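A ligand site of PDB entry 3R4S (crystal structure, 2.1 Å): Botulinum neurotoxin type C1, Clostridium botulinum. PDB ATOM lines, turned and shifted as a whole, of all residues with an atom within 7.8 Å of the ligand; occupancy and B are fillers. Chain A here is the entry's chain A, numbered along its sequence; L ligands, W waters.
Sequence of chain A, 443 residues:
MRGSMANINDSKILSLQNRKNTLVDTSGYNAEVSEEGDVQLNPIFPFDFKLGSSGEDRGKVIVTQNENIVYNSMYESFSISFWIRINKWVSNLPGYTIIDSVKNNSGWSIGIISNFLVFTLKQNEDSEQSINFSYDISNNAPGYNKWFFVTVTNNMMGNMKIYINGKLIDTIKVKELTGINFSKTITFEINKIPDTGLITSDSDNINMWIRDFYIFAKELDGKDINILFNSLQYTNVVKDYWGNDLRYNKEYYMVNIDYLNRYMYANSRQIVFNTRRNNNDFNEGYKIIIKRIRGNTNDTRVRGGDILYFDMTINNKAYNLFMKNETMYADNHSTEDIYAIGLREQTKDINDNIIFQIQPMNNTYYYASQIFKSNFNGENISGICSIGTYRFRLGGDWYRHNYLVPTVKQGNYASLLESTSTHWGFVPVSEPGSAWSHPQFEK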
ATOM      1  N   ASN A 249      18.492 -18.785 -14.040  1.00  0.00           N
ATOM      2  CA  ASN A 249      18.431 -18.869 -15.502  1.00  0.00           C
ATOM      3  C   ASN A 249      19.611 -19.607 -16.117  1.00  0.00           C
ATOM      4  O   ASN A 249      20.037 -19.292 -17.232  1.00  0.00           O
ATOM      5  CB  ASN A 249      18.336 -17.478 -16.122  1.00  0.00           C
ATOM      6  CG  ASN A 249      17.223 -16.647 -15.535  1.00  0.00           C
ATOM      7  OD1 ASN A 249      16.200 -17.183 -15.071  1.00  0.00           O
ATOM      8  ND2 ASN A 249      17.396 -15.338 -15.533  1.00  0.00           N
ATOM      9  N   ILE A 289      16.662 -25.532 -14.143  1.00  0.00           N
ATOM     10  CA  ILE A 289      17.015 -24.129 -14.201  1.00  0.00           C
ATOM     11  C   ILE A 289      16.289 -23.473 -13.031  1.00  0.00           C
ATOM     12  O   ILE A 289      15.109 -23.743 -12.803  1.00  0.00           O
ATOM     13  CB  ILE A 289      16.532 -23.483 -15.524  1.00  0.00           C
ATOM     14  CG1 ILE A 289      17.285 -24.110 -16.705  1.00  0.00           C
ATOM     15  CG2 ILE A 289      16.738 -21.977 -15.480  1.00  0.00           C
ATOM     16  CD1 ILE A 289      16.845 -23.571 -18.064  1.00  0.00           C
ATOM     17  N   ILE A 290      17.004 -22.629 -12.298  1.00  0.00           N
ATOM     18  CA  ILE A 290      16.444 -21.961 -11.127  1.00  0.00           C
ATOM     19  C   ILE A 290      15.842 -20.623 -11.537  1.00  0.00           C
ATOM     20  O   ILE A 290      16.487 -19.849 -12.226  1.00  0.00           O
ATOM     21  CB  ILE A 290      17.529 -21.714 -10.060  1.00  0.00           C
ATOM     22  CG1 ILE A 290      18.339 -22.995  -9.806  1.00  0.00           C
ATOM     23  CG2 ILE A 290      16.908 -21.197  -8.762  1.00  0.00           C
ATOM     24  CD1 ILE A 290      19.547 -22.809  -8.937  1.00  0.00           C
ATOM     25  N   LYS A 291      14.616 -20.349 -11.107  1.00  0.00           N
ATOM     26  CA  LYS A 291      13.955 -19.087 -11.464  1.00  0.00           C
ATOM     27  C   LYS A 291      13.650 -18.272 -10.216  1.00  0.00           C
ATOM     28  O   LYS A 291      13.112 -18.780  -9.241  1.00  0.00           O
ATOM     29  CB  LYS A 291      12.653 -19.342 -12.229  1.00  0.00           C
ATOM     30  CG  LYS A 291      12.788 -20.307 -13.391  1.00  0.00           C
ATOM     31  CD  LYS A 291      13.667 -19.748 -14.502  1.00  0.00           C
ATOM     32  CE  LYS A 291      13.041 -18.515 -15.156  1.00  0.00           C
ATOM     33  NZ  LYS A 291      13.900 -17.985 -16.275  1.00  0.00           N
ATOM     34  N   ARG A 292      13.969 -16.987 -10.276  1.00  0.00           N
ATOM     35  CA  ARG A 292      13.782 -16.115  -9.122  1.00  0.00           C
ATOM     36  C   ARG A 292      12.356 -15.596  -8.977  1.00  0.00           C
ATOM     37  O   ARG A 292      11.722 -15.183  -9.949  1.00  0.00           O
ATOM     38  CB  ARG A 292      14.751 -14.938  -9.195  1.00  0.00           C
ATOM     39  CG  ARG A 292      14.767 -14.057  -7.930  1.00  0.00           C
ATOM     40  CD  ARG A 292      15.761 -12.890  -8.057  1.00  0.00           C
ATOM     41  NE  ARG A 292      15.385 -12.008  -9.158  1.00  0.00           N
ATOM     42  CZ  ARG A 292      16.228 -11.494 -10.046  1.00  0.00           C
ATOM     43  NH1 ARG A 292      17.528 -11.771  -9.985  1.00  0.00           N
ATOM     44  NH2 ARG A 292      15.767 -10.706 -11.008  1.00  0.00           N
ATOM     45  N   TYR A 309      11.673 -20.948  -7.775  1.00  0.00           N
ATOM     46  CA  TYR A 309      11.090 -22.216  -8.195  1.00  0.00           C
ATOM     47  C   TYR A 309      12.029 -22.835  -9.217  1.00  0.00           C
ATOM     48  O   TYR A 309      13.007 -22.210  -9.624  1.00  0.00           O
ATOM     49  CB  TYR A 309       9.671 -22.037  -8.763  1.00  0.00           C
ATOM     50  CG  TYR A 309       9.607 -21.203 -10.031  1.00  0.00           C
ATOM     51  CD1 TYR A 309       9.676 -21.810 -11.287  1.00  0.00           C
ATOM     52  CD2 TYR A 309       9.491 -19.822  -9.972  1.00  0.00           C
ATOM     53  CE1 TYR A 309       9.600 -21.051 -12.452  1.00  0.00           C
ATOM     54  CE2 TYR A 309       9.420 -19.050 -11.135  1.00  0.00           C
ATOM     55  CZ  TYR A 309       9.476 -19.669 -12.374  1.00  0.00           C
ATOM     56  OH  TYR A 309       9.427 -18.900 -13.529  1.00  0.00           O
ATOM     57  N   PHE A 310      11.749 -24.075  -9.626  1.00  0.00           N
ATOM     58  CA  PHE A 310      12.643 -24.788 -10.526  1.00  0.00           C
ATOM     59  C   PHE A 310      11.926 -25.242 -11.812  1.00  0.00           C
ATOM     60  O   PHE A 310      10.821 -25.786 -11.745  1.00  0.00           O
ATOM     61  CB  PHE A 310      13.220 -26.031  -9.826  1.00  0.00           C
ATOM     62  CG  PHE A 310      13.982 -25.712  -8.554  1.00  0.00           C
ATOM     63  CD1 PHE A 310      15.328 -25.364  -8.610  1.00  0.00           C
ATOM     64  CD2 PHE A 310      13.362 -25.797  -7.313  1.00  0.00           C
ATOM     65  CE1 PHE A 310      16.040 -25.086  -7.432  1.00  0.00           C
ATOM     66  CE2 PHE A 310      14.065 -25.522  -6.138  1.00  0.00           C
ATOM     67  CZ  PHE A 310      15.405 -25.155  -6.197  1.00  0.00           C
ATOM     68  N   ASP A 311      12.564 -25.032 -12.960  1.00  0.00           N
ATOM     69  CA  ASP A 311      12.090 -25.556 -14.247  1.00  0.00           C
ATOM     70  C   ASP A 311      12.917 -26.755 -14.674  1.00  0.00           C
ATOM     71  O   ASP A 311      14.124 -26.816 -14.437  1.00  0.00           O
ATOM     72  CB  ASP A 311      12.225 -24.505 -15.332  1.00  0.00           C
ATOM     73  CG  ASP A 311      11.268 -23.361 -15.159  1.00  0.00           C
ATOM     74  OD1 ASP A 311      10.242 -23.559 -14.464  1.00  0.00           O
ATOM     75  OD2 ASP A 311      11.527 -22.281 -15.713  1.00  0.00           O
ATOM     76  N   ALA A 318       8.368 -27.804 -21.106  1.00  0.00           N
ATOM     77  CA  ALA A 318       8.939 -27.236 -19.878  1.00  0.00           C
ATOM     78  C   ALA A 318       8.001 -27.421 -18.687  1.00  0.00           C
ATOM     79  O   ALA A 318       6.835 -27.024 -18.739  1.00  0.00           O
ATOM     80  CB  ALA A 318       9.274 -25.754 -20.084  1.00  0.00           C
ATOM     81  N   TYR A 319       8.519 -28.017 -17.619  1.00  0.00           N
ATOM     82  CA  TYR A 319       7.758 -28.246 -16.400  1.00  0.00           C
ATOM     83  C   TYR A 319       8.268 -27.407 -15.221  1.00  0.00           C
ATOM     84  O   TYR A 319       9.338 -26.811 -15.280  1.00  0.00           O
ATOM     85  CB  TYR A 319       7.860 -29.706 -15.992  1.00  0.00           C
ATOM     86  CG  TYR A 319       7.392 -30.703 -17.035  1.00  0.00           C
ATOM     87  CD1 TYR A 319       6.099 -31.209 -17.021  1.00  0.00           C
ATOM     88  CD2 TYR A 319       8.257 -31.161 -18.024  1.00  0.00           C
ATOM     89  CE1 TYR A 319       5.669 -32.138 -17.964  1.00  0.00           C
ATOM     90  CE2 TYR A 319       7.848 -32.083 -18.970  1.00  0.00           C
ATOM     91  CZ  TYR A 319       6.551 -32.567 -18.936  1.00  0.00           C
ATOM     92  OH  TYR A 319       6.138 -33.489 -19.873  1.00  0.00           O
ATOM     93  N   ASN A 320       7.497 -27.383 -14.138  1.00  0.00           N
ATOM     94  CA  ASN A 320       7.953 -26.917 -12.836  1.00  0.00           C
ATOM     95  C   ASN A 320       8.080 -28.118 -11.926  1.00  0.00           C
ATOM     96  O   ASN A 320       7.236 -29.027 -11.968  1.00  0.00           O
ATOM     97  CB  ASN A 320       6.934 -25.973 -12.192  1.00  0.00           C
ATOM     98  CG  ASN A 320       6.692 -24.707 -12.986  1.00  0.00           C
ATOM     99  OD1 ASN A 320       5.548 -24.304 -13.191  1.00  0.00           O
ATOM    100  ND2 ASN A 320       7.769 -24.066 -13.429  1.00  0.00           N
ATOM    101  N   ARG A 344       5.026 -30.676 -13.075  1.00  0.00           N
ATOM    102  CA  ARG A 344       3.740 -30.235 -13.594  1.00  0.00           C
ATOM    103  C   ARG A 344       3.951 -29.193 -14.692  1.00  0.00           C
ATOM    104  O   ARG A 344       4.932 -28.435 -14.680  1.00  0.00           O
ATOM    105  CB  ARG A 344       2.880 -29.642 -12.487  1.00  0.00           C
ATOM    106  CG  ARG A 344       3.483 -28.394 -11.865  1.00  0.00           C
ATOM    107  CD  ARG A 344       2.515 -27.701 -10.930  1.00  0.00           C
ATOM    108  NE  ARG A 344       1.355 -27.181 -11.647  1.00  0.00           N
ATOM    109  CZ  ARG A 344       0.369 -26.491 -11.073  1.00  0.00           C
ATOM    110  NH1 ARG A 344       0.414 -26.233  -9.769  1.00  0.00           N
ATOM    111  NH2 ARG A 344      -0.644 -26.052 -11.796  1.00  0.00           N
ATOM    112  N   GLU A 345       3.014 -29.138 -15.618  1.00  0.00           N
ATOM    113  CA  GLU A 345       3.067 -28.190 -16.713  1.00  0.00           C
ATOM    114  C   GLU A 345       3.057 -26.771 -16.172  1.00  0.00           C
ATOM    115  O   GLU A 345       2.327 -26.467 -15.236  1.00  0.00           O
ATOM    116  CB  GLU A 345       1.879 -28.380 -17.659  1.00  0.00           C
ATOM    117  CG  GLU A 345       1.963 -29.635 -18.495  1.00  0.00           C
ATOM    118  CD  GLU A 345       0.774 -29.771 -19.432  1.00  0.00           C
ATOM    119  OE1 GLU A 345       0.302 -28.732 -19.938  1.00  0.00           O
ATOM    120  OE2 GLU A 345       0.322 -30.913 -19.640  1.00  0.00           O
ATOM    121  N   GLN A 346       3.858 -25.915 -16.790  1.00  0.00           N
ATOM    122  CA  GLN A 346       3.916 -24.516 -16.405  1.00  0.00           C
ATOM    123  C   GLN A 346       2.571 -23.844 -16.648  1.00  0.00           C
ATOM    124  O   GLN A 346       1.818 -24.254 -17.530  1.00  0.00           O
ATOM    125  CB  GLN A 346       5.007 -23.791 -17.199  1.00  0.00           C
ATOM    126  CG  GLN A 346       6.395 -24.295 -16.908  1.00  0.00           C
ATOM    127  CD  GLN A 346       7.459 -23.480 -17.606  1.00  0.00           C
ATOM    128  OE1 GLN A 346       7.152 -22.647 -18.453  1.00  0.00           O
ATOM    129  NE2 GLN A 346       8.721 -23.710 -17.260  1.00  0.00           N
ATOM    130  N   THR A 347       2.267 -22.827 -15.864  1.00  0.00           N
ATOM    131  CA  THR A 347       1.056 -22.051 -16.056  1.00  0.00           C
ATOM    132  C   THR A 347       1.437 -20.588 -16.126  1.00  0.00           C
ATOM    133  O   THR A 347       2.611 -20.229 -15.927  1.00  0.00           O
ATOM    134  CB  THR A 347       0.027 -22.251 -14.911  1.00  0.00           C
ATOM    135  OG1 THR A 347       0.618 -21.875 -13.663  1.00  0.00           O
ATOM    136  CG2 THR A 347      -0.432 -23.686 -14.840  1.00  0.00           C
ATOM    137  N   LYS A 348       0.472 -19.734 -16.415  1.00  0.00           N
ATOM    138  CA  LYS A 348       0.726 -18.303 -16.566  1.00  0.00           C
ATOM    139  C   LYS A 348       1.122 -17.691 -15.224  1.00  0.00           C
ATOM    140  O   LYS A 348       1.959 -16.792 -15.152  1.00  0.00           O
ATOM    141  CB  LYS A 348      -0.513 -17.608 -17.133  1.00  0.00           C
ATOM    142  CG  LYS A 348      -0.343 -16.103 -17.317  1.00  0.00           C
ATOM    143  CD  LYS A 348      -1.698 -15.411 -17.468  1.00  0.00           C
ATOM    144  CE  LYS A 348      -1.573 -13.890 -17.433  1.00  0.00           C
ATOM    145  NZ  LYS A 348      -0.861 -13.344 -18.631  1.00  0.00           N
ATOM    146  N   ASP A 349       0.512 -18.190 -14.159  1.00  0.00           N
ATOM    147  CA  ASP A 349       0.774 -17.675 -12.816  1.00  0.00           C
ATOM    148  C   ASP A 349       1.564 -18.669 -11.970  1.00  0.00           C
ATOM    149  O   ASP A 349       1.419 -19.875 -12.144  1.00  0.00           O
ATOM    150  CB  ASP A 349      -0.544 -17.342 -12.121  1.00  0.00           C
ATOM    151  CG  ASP A 349      -1.308 -16.222 -12.807  1.00  0.00           C
ATOM    152  OD1 ASP A 349      -0.666 -15.199 -13.146  1.00  0.00           O
ATOM    153  OD2 ASP A 349      -2.535 -16.363 -12.996  1.00  0.00           O
ATOM    154  N   ILE A 350       2.393 -18.146 -11.071  1.00  0.00           N
ATOM    155  CA  ILE A 350       3.138 -18.971 -10.127  1.00  0.00           C
ATOM    156  C   ILE A 350       2.178 -19.615  -9.132  1.00  0.00           C
ATOM    157  O   ILE A 350       1.557 -18.922  -8.330  1.00  0.00           O
ATOM    158  CB  ILE A 350       4.159 -18.144  -9.316  1.00  0.00           C
ATOM    159  CG1 ILE A 350       5.022 -17.266 -10.232  1.00  0.00           C
ATOM    160  CG2 ILE A 350       5.023 -19.044  -8.432  1.00  0.00           C
ATOM    161  CD1 ILE A 350       5.843 -18.034 -11.214  1.00  0.00           C
ATOM    162  N   ASN A 351       2.055 -20.943  -9.157  1.00  0.00           N
ATOM    163  CA  ASN A 351       1.264 -21.625  -8.150  1.00  0.00           C
ATOM    164  C   ASN A 351       2.054 -21.923  -6.871  1.00  0.00           C
ATOM    165  O   ASN A 351       3.250 -22.197  -6.926  1.00  0.00           O
ATOM    166  CB  ASN A 351       0.678 -22.923  -8.710  1.00  0.00           C
ATOM    167  CG  ASN A 351      -0.464 -22.677  -9.675  1.00  0.00           C
ATOM    168  OD1 ASN A 351      -0.305 -22.772 -10.901  1.00  0.00           O
ATOM    169  ND2 ASN A 351      -1.636 -22.337  -9.128  1.00  0.00           N
ATOM    170  N   ILE A 354       4.785 -24.799  -6.278  1.00  0.00           N
ATOM    171  CA  ILE A 354       6.121 -24.840  -6.893  1.00  0.00           C
ATOM    172  C   ILE A 354       7.125 -23.944  -6.165  1.00  0.00           C
ATOM    173  O   ILE A 354       8.316 -23.914  -6.537  1.00  0.00           O
ATOM    174  CB  ILE A 354       6.119 -24.407  -8.370  1.00  0.00           C
ATOM    175  CG1 ILE A 354       5.969 -22.890  -8.475  1.00  0.00           C
ATOM    176  CG2 ILE A 354       5.058 -25.194  -9.175  1.00  0.00           C
ATOM    177  CD1 ILE A 354       6.187 -22.364  -9.877  1.00  0.00           C
HETATM  178  C1  LIG L   1       9.721 -19.691 -16.886  1.00  0.00           C
HETATM  179  C2  LIG L   1       8.810 -18.489 -17.007  1.00  0.00           C
HETATM  180  C3  LIG L   1       8.530 -18.145 -18.473  1.00  0.00           C
HETATM  181  C4  LIG L   1       7.507 -19.059 -19.133  1.00  0.00           C
HETATM  182  C5  LIG L   1       6.296 -19.237 -18.242  1.00  0.00           C
HETATM  183  C6  LIG L   1       6.750 -19.728 -16.878  1.00  0.00           C
HETATM  184  C7  LIG L   1       5.605 -20.002 -15.917  1.00  0.00           C
HETATM  185  C8  LIG L   1       6.145 -20.467 -14.562  1.00  0.00           C
HETATM  186  C9  LIG L   1       5.019 -21.001 -13.688  1.00  0.00           C
HETATM  187  C10 LIG L   1       4.281 -20.158 -19.215  1.00  0.00           C
HETATM  188  C11 LIG L   1       3.609 -21.363 -19.821  1.00  0.00           C
HETATM  189  N1  LIG L   1       5.555 -20.326 -18.843  1.00  0.00           N
HETATM  190  O1  LIG L   1       9.695 -20.336 -15.805  1.00  0.00           O
HETATM  191  O2  LIG L   1      10.470 -19.992 -17.846  1.00  0.00           O
HETATM  192  O3  LIG L   1       9.470 -17.391 -16.383  1.00  0.00           O
HETATM  193  O4  LIG L   1       7.104 -18.493 -20.381  1.00  0.00           O
HETATM  194  O5  LIG L   1       7.605 -18.751 -16.284  1.00  0.00           O
HETATM  195  O6  LIG L   1       4.854 -18.799 -15.718  1.00  0.00           O
HETATM  196  O7  LIG L   1       7.149 -21.480 -14.750  1.00  0.00           O
HETATM  197  O8  LIG L   1       4.635 -22.280 -14.202  1.00  0.00           O
HETATM  198  O9  LIG L   1       3.708 -19.095 -19.074  1.00  0.00           O
HETATM  199  O   HOH W   1       7.965 -15.105 -16.243  1.00  0.00           O
HETATM  200  O   HOH W   2      10.672 -22.470 -18.752  1.00  0.00           O
HETATM  201  O   HOH W   3      12.196 -18.595 -19.353  1.00  0.00           O
HETATM  202  O   HOH W   4       2.554 -22.648 -11.469  1.00  0.00           O
HETATM  203  O   HOH W   5       9.032 -16.279 -13.440  1.00  0.00           O
HETATM  204  O   HOH W   6       5.928 -16.159 -14.592  1.00  0.00           O
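An oxygen (O6) of the ligand sits at hydrogen-bond distance from the backbone carbonyl oxygen (O) of Thr 347 (2.7 Å).
The side-chain hydroxyl (OH) of Tyr 309 sits at hydrogen-bond distance from an oxygen (O1) of the ligand.
OE1 of Gln 346 lies within hydrogen-bond range of N1 of the ligand (2.8 Å).
OD1 of Asn 320 lies within hydrogen-bond range of O8 of the ligand, at 2.4 Å.
OD2 of Asp 311 lies close to O1 of the ligand.
The backbone NH (N) of Thr 347 lies within hydrogen-bond range of an oxygen (O8) of the ligand, at 2.9 Å.
O of Ile 289 sits at hydrogen-bond distance from N of Asp 311, at 2.9 Å.
N of Lys 291 is in hydrogen-bond range of O of Tyr 309 (2.9 Å).
NZ of Lys 291 lies within hydrogen-bond range of OD1 of Asn 249, at 2.7 Å.
The side-chain hydroxyl (OG1) of Thr 347 lies within hydrogen-bond range of the backbone carbonyl oxygen (O) of Asp 349 (2.6 Å).
The side-chain hydroxyl of Thr 347 lies within hydrogen-bond range of the side-chain amide oxygen of Asn 351 (3.0 Å).
OD1 of Asp 311 lies within hydrogen-bond range of ND2 of Asn 320.
The backbone carbonyl oxygen of Arg 344 sits at hydrogen-bond distance from the backbone NH of Asn 320, at 2.8 Å.
The side-chain carboxylate of Asp 311 lies within hydrogen-bond range of the side-chain amide nitrogen of Gln 346, 3.2 Å away.
Lys 291 touches the ligand (CE to O1, 3.9 Å).
Lys 348 touches the ligand (O to O6, 3.6 Å).
Ile 350 touches the ligand (CD1 to C9, 3.95 Å).
Hydrophobic or aromatic side chains that line the ligand: Tyr 309 and Ile 350.
Eight residues have an atom within 4 Å of the ligand: Lys 291, Tyr 309, Asp 311, Asn 320, Gln 346, Thr 347, Lys 348 and Ile 350.
The nearest printed residue that does not touch the ligand is Asp 349 (4.1 Å).
Water W2 lies within hydrogen-bond range of an oxygen (O2) of the ligand, the side-chain amide nitrogen of Gln 346 and the side-chain carboxylate of Asp 311.
Water W5 bridges OH of Tyr 309 (2.7 Å) and O3 of the ligand (3.2 Å).
Water W4 lies within hydrogen-bond range of N of Asn 351 (2.9 Å), OG1 of Thr 347 (3.0 Å), O of Asp 349 (3.1 Å) and O8 of the ligand (3.5 Å).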
